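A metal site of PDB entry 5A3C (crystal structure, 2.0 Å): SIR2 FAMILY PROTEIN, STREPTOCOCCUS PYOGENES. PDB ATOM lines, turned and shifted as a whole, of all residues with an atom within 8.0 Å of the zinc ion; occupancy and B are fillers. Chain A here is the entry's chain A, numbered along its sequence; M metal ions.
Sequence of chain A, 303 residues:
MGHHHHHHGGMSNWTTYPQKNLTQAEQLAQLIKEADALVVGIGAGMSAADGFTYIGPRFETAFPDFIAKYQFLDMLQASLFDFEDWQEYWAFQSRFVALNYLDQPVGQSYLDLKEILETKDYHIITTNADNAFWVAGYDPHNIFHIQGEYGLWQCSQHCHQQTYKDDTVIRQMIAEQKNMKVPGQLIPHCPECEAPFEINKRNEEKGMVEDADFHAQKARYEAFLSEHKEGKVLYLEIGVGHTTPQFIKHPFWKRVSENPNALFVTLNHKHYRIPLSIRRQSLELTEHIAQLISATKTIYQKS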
ATOM      1  N   GLN A 154      -1.341 -28.071  12.647  1.00  0.00           N
ATOM      2  CA  GLN A 154      -2.244 -26.979  13.018  1.00  0.00           C
ATOM      3  C   GLN A 154      -3.578 -27.581  13.384  1.00  0.00           C
ATOM      4  O   GLN A 154      -3.897 -28.712  12.992  1.00  0.00           O
ATOM      5  CB  GLN A 154      -2.423 -25.982  11.855  1.00  0.00           C
ATOM      6  CG  GLN A 154      -3.269 -26.505  10.697  1.00  0.00           C
ATOM      7  CD  GLN A 154      -3.285 -25.603   9.460  1.00  0.00           C
ATOM      8  OE1 GLN A 154      -2.520 -24.640   9.342  1.00  0.00           O
ATOM      9  NE2 GLN A 154      -4.157 -25.932   8.515  1.00  0.00           N
ATOM     10  N   CYS A 155      -4.373 -26.822  14.145  1.00  0.00           N
ATOM     11  CA  CYS A 155      -5.719 -27.239  14.495  1.00  0.00           C
ATOM     12  C   CYS A 155      -6.538 -27.287  13.221  1.00  0.00           C
ATOM     13  O   CYS A 155      -6.480 -26.372  12.413  1.00  0.00           O
ATOM     14  CB  CYS A 155      -6.343 -26.248  15.490  1.00  0.00           C
ATOM     15  SG  CYS A 155      -8.104 -26.562  15.823  1.00  0.00           S
ATOM     16  N   SER A 156      -7.299 -28.371  13.032  1.00  0.00           N
ATOM     17  CA  SER A 156      -8.123 -28.515  11.830  1.00  0.00           C
ATOM     18  C   SER A 156      -9.220 -27.464  11.762  1.00  0.00           C
ATOM     19  O   SER A 156      -9.761 -27.178  10.678  1.00  0.00           O
ATOM     20  CB  SER A 156      -8.726 -29.917  11.738  1.00  0.00           C
ATOM     21  OG  SER A 156      -9.461 -30.239  12.904  1.00  0.00           O
ATOM     22  N   GLN A 157      -9.536 -26.862  12.905  1.00  0.00           N
ATOM     23  CA  GLN A 157     -10.514 -25.769  12.974  1.00  0.00           C
ATOM     24  C   GLN A 157      -9.843 -24.407  13.019  1.00  0.00           C
ATOM     25  O   GLN A 157     -10.532 -23.393  13.081  1.00  0.00           O
ATOM     26  CB  GLN A 157     -11.373 -25.937  14.219  1.00  0.00           C
ATOM     27  CG  GLN A 157     -12.095 -27.271  14.278  1.00  0.00           C
ATOM     28  CD  GLN A 157     -13.443 -27.208  13.610  1.00  0.00           C
ATOM     29  OE1 GLN A 157     -14.366 -26.570  14.132  1.00  0.00           O
ATOM     30  NE2 GLN A 157     -13.579 -27.872  12.470  1.00  0.00           N
ATOM     31  N   HIS A 158      -8.514 -24.387  12.996  1.00  0.00           N
ATOM     32  CA  HIS A 158      -7.750 -23.142  13.029  1.00  0.00           C
ATOM     33  C   HIS A 158      -8.180 -22.275  14.220  1.00  0.00           C
ATOM     34  O   HIS A 158      -8.269 -21.051  14.095  1.00  0.00           O
ATOM     35  CB  HIS A 158      -7.959 -22.326  11.733  1.00  0.00           C
ATOM     36  CG  HIS A 158      -7.563 -23.027  10.476  1.00  0.00           C
ATOM     37  ND1 HIS A 158      -6.958 -22.368   9.426  1.00  0.00           N
ATOM     38  CD2 HIS A 158      -7.681 -24.328  10.086  1.00  0.00           C
ATOM     39  CE1 HIS A 158      -6.719 -23.226   8.447  1.00  0.00           C
ATOM     40  NE2 HIS A 158      -7.151 -24.419   8.826  1.00  0.00           N
ATOM     41  N   CYS A 159      -8.441 -22.908  15.355  1.00  0.00           N
ATOM     42  CA  CYS A 159      -9.049 -22.207  16.500  1.00  0.00           C
ATOM     43  C   CYS A 159      -8.081 -21.231  17.162  1.00  0.00           C
ATOM     44  O   CYS A 159      -8.497 -20.295  17.827  1.00  0.00           O
ATOM     45  CB  CYS A 159      -9.619 -23.183  17.535  1.00  0.00           C
ATOM     46  SG  CYS A 159      -8.447 -23.854  18.725  1.00  0.00           S
ATOM     47  N   HIS A 160      -6.772 -21.448  16.981  1.00  0.00           N
ATOM     48  CA  HIS A 160      -5.768 -20.517  17.476  1.00  0.00           C
ATOM     49  C   HIS A 160      -4.503 -20.583  16.609  1.00  0.00           C
ATOM     50  O   HIS A 160      -4.237 -21.604  15.969  1.00  0.00           O
ATOM     51  CB  HIS A 160      -5.473 -20.789  18.967  1.00  0.00           C
ATOM     52  CG  HIS A 160      -4.790 -22.097  19.224  1.00  0.00           C
ATOM     53  ND1 HIS A 160      -5.386 -23.313  18.977  1.00  0.00           N
ATOM     54  CD2 HIS A 160      -3.560 -22.379  19.724  1.00  0.00           C
ATOM     55  CE1 HIS A 160      -4.550 -24.286  19.293  1.00  0.00           C
ATOM     56  NE2 HIS A 160      -3.434 -23.748  19.747  1.00  0.00           N
ATOM     57  N   TYR A 164       2.368 -26.914  15.923  1.00  0.00           N
ATOM     58  CA  TYR A 164       2.875 -27.937  16.824  1.00  0.00           C
ATOM     59  C   TYR A 164       3.656 -28.945  16.013  1.00  0.00           C
ATOM     60  O   TYR A 164       3.453 -29.042  14.802  1.00  0.00           O
ATOM     61  CB  TYR A 164       1.705 -28.652  17.520  1.00  0.00           C
ATOM     62  CG  TYR A 164       0.859 -27.746  18.383  1.00  0.00           C
ATOM     63  CD1 TYR A 164      -0.113 -26.933  17.822  1.00  0.00           C
ATOM     64  CD2 TYR A 164       1.049 -27.679  19.763  1.00  0.00           C
ATOM     65  CE1 TYR A 164      -0.883 -26.092  18.602  1.00  0.00           C
ATOM     66  CE2 TYR A 164       0.277 -26.847  20.548  1.00  0.00           C
ATOM     67  CZ  TYR A 164      -0.695 -26.062  19.962  1.00  0.00           C
ATOM     68  OH  TYR A 164      -1.460 -25.227  20.736  1.00  0.00           O
ATOM     69  N   HIS A 189      -4.821 -34.480  18.910  1.00  0.00           N
ATOM     70  CA  HIS A 189      -5.902 -33.485  18.995  1.00  0.00           C
ATOM     71  C   HIS A 189      -5.439 -32.139  19.535  1.00  0.00           C
ATOM     72  O   HIS A 189      -4.577 -32.071  20.395  1.00  0.00           O
ATOM     73  CB  HIS A 189      -7.014 -34.012  19.891  1.00  0.00           C
ATOM     74  CG  HIS A 189      -7.769 -35.149  19.282  1.00  0.00           C
ATOM     75  ND1 HIS A 189      -7.471 -36.473  19.532  1.00  0.00           N
ATOM     76  CD2 HIS A 189      -8.795 -35.160  18.401  1.00  0.00           C
ATOM     77  CE1 HIS A 189      -8.295 -37.246  18.855  1.00  0.00           C
ATOM     78  NE2 HIS A 189      -9.098 -36.468  18.146  1.00  0.00           N
ATOM     79  N   CYS A 190      -6.032 -31.081  18.995  1.00  0.00           N
ATOM     80  CA  CYS A 190      -5.802 -29.706  19.444  1.00  0.00           C
ATOM     81  C   CYS A 190      -6.114 -29.591  20.926  1.00  0.00           C
ATOM     82  O   CYS A 190      -7.202 -29.937  21.358  1.00  0.00           O
ATOM     83  CB  CYS A 190      -6.684 -28.762  18.626  1.00  0.00           C
ATOM     84  SG  CYS A 190      -6.794 -27.049  19.188  1.00  0.00           S
ATOM     85  N   PRO A 191      -5.148 -29.122  21.736  1.00  0.00           N
ATOM     86  CA  PRO A 191      -5.392 -29.011  23.172  1.00  0.00           C
ATOM     87  C   PRO A 191      -6.367 -27.903  23.590  1.00  0.00           C
ATOM     88  O   PRO A 191      -6.782 -27.885  24.745  1.00  0.00           O
ATOM     89  CB  PRO A 191      -3.997 -28.744  23.763  1.00  0.00           C
ATOM     90  CG  PRO A 191      -3.216 -28.153  22.645  1.00  0.00           C
ATOM     91  CD  PRO A 191      -3.772 -28.732  21.371  1.00  0.00           C
ATOM     92  N   GLU A 192      -6.723 -26.999  22.685  1.00  0.00           N
ATOM     93  CA  GLU A 192      -7.648 -25.918  22.982  1.00  0.00           C
ATOM     94  C   GLU A 192      -9.099 -26.307  22.686  1.00  0.00           C
ATOM     95  O   GLU A 192      -9.997 -25.962  23.461  1.00  0.00           O
ATOM     96  CB  GLU A 192      -7.324 -24.681  22.143  1.00  0.00           C
ATOM     97  CG  GLU A 192      -5.959 -24.073  22.408  1.00  0.00           C
ATOM     98  CD  GLU A 192      -5.890 -23.339  23.729  1.00  0.00           C
ATOM     99  OE1 GLU A 192      -6.829 -22.588  24.055  1.00  0.00           O
ATOM    100  OE2 GLU A 192      -4.875 -23.507  24.430  1.00  0.00           O
ATOM    101  N   CYS A 193      -9.334 -26.978  21.570  1.00  0.00           N
ATOM    102  CA  CYS A 193     -10.700 -27.229  21.117  1.00  0.00           C
ATOM    103  C   CYS A 193     -11.018 -28.718  20.914  1.00  0.00           C
ATOM    104  O   CYS A 193     -12.151 -29.061  20.619  1.00  0.00           O
ATOM    105  CB  CYS A 193     -10.974 -26.451  19.824  1.00  0.00           C
ATOM    106  SG  CYS A 193     -10.284 -27.221  18.340  1.00  0.00           S
ATOM    107  N   GLU A 194     -10.002 -29.569  21.048  1.00  0.00           N
ATOM    108  CA  GLU A 194     -10.137 -31.027  20.890  1.00  0.00           C
ATOM    109  C   GLU A 194     -10.423 -31.523  19.466  1.00  0.00           C
ATOM    110  O   GLU A 194     -10.629 -32.717  19.255  1.00  0.00           O
ATOM    111  CB  GLU A 194     -11.148 -31.602  21.898  1.00  0.00           C
ATOM    112  CG  GLU A 194     -10.602 -31.660  23.321  1.00  0.00           C
ATOM    113  CD  GLU A 194      -9.395 -32.563  23.433  1.00  0.00           C
ATOM    114  OE1 GLU A 194      -9.552 -33.782  23.177  1.00  0.00           O
ATOM    115  OE2 GLU A 194      -8.286 -32.079  23.752  1.00  0.00           O
ATOM    116  N   ALA A 195     -10.406 -30.632  18.469  1.00  0.00           N
ATOM    117  CA  ALA A 195     -10.504 -31.064  17.086  1.00  0.00           C
ATOM    118  C   ALA A 195      -9.176 -31.757  16.705  1.00  0.00           C
ATOM    119  O   ALA A 195      -8.143 -31.507  17.327  1.00  0.00           O
ATOM    120  CB  ALA A 195     -10.796 -29.891  16.181  1.00  0.00           C
ATOM    121  N   PRO A 196      -9.200 -32.670  15.720  1.00  0.00           N
ATOM    122  CA  PRO A 196      -7.923 -33.291  15.346  1.00  0.00           C
ATOM    123  C   PRO A 196      -6.903 -32.306  14.770  1.00  0.00           C
ATOM    124  O   PRO A 196      -7.291 -31.360  14.083  1.00  0.00           O
ATOM    125  CB  PRO A 196      -8.338 -34.291  14.265  1.00  0.00           C
ATOM    126  CG  PRO A 196      -9.786 -34.548  14.507  1.00  0.00           C
ATOM    127  CD  PRO A 196     -10.337 -33.242  14.994  1.00  0.00           C
ATOM    128  N   PHE A 197      -5.614 -32.522  15.054  1.00  0.00           N
ATOM    129  CA  PHE A 197      -4.580 -31.813  14.304  1.00  0.00           C
ATOM    130  C   PHE A 197      -4.648 -32.245  12.838  1.00  0.00           C
ATOM    131  O   PHE A 197      -5.113 -33.342  12.522  1.00  0.00           O
ATOM    132  CB  PHE A 197      -3.176 -32.075  14.867  1.00  0.00           C
ATOM    133  CG  PHE A 197      -2.824 -31.241  16.068  1.00  0.00           C
ATOM    134  CD1 PHE A 197      -2.893 -29.856  16.006  1.00  0.00           C
ATOM    135  CD2 PHE A 197      -2.411 -31.834  17.248  1.00  0.00           C
ATOM    136  CE1 PHE A 197      -2.569 -29.085  17.108  1.00  0.00           C
ATOM    137  CE2 PHE A 197      -2.079 -31.068  18.360  1.00  0.00           C
ATOM    138  CZ  PHE A 197      -2.158 -29.685  18.276  1.00  0.00           C
HETATM  139 ZN    ZN M   1      -8.321 -26.158  18.097  1.00  0.00          ZN
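The side-chain sulfur of Cys 190 sits close to the backbone NH of Glu 192 (3.5 Å). O of Ala 195 lies within hydrogen-bond range of N of Cys 190 (2.7 Å). The backbone NH (N) of Ala 195 sits close to the side-chain sulfur (SG) of Cys 193 (3.4 Å). N of Gln 157 sits close to SG of Cys 155, at 3.3 Å. The backbone NH of His 158 sits close to the side-chain sulfur of Cys 155, 3.6 Å away. The side-chain sulfur of Cys 159 sits close to a ring nitrogen (ND1) of His 160, 3.1 Å away.
SG of Cys 190 is bound to the zinc ion, at 2.1 Å. The side-chain sulfur (SG) of Cys 193 binds the zinc ion, 2.2 Å away. SG of Cys 155 binds the zinc ion (2.3 Å). The zinc ion is bound by SG of Cys 159.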
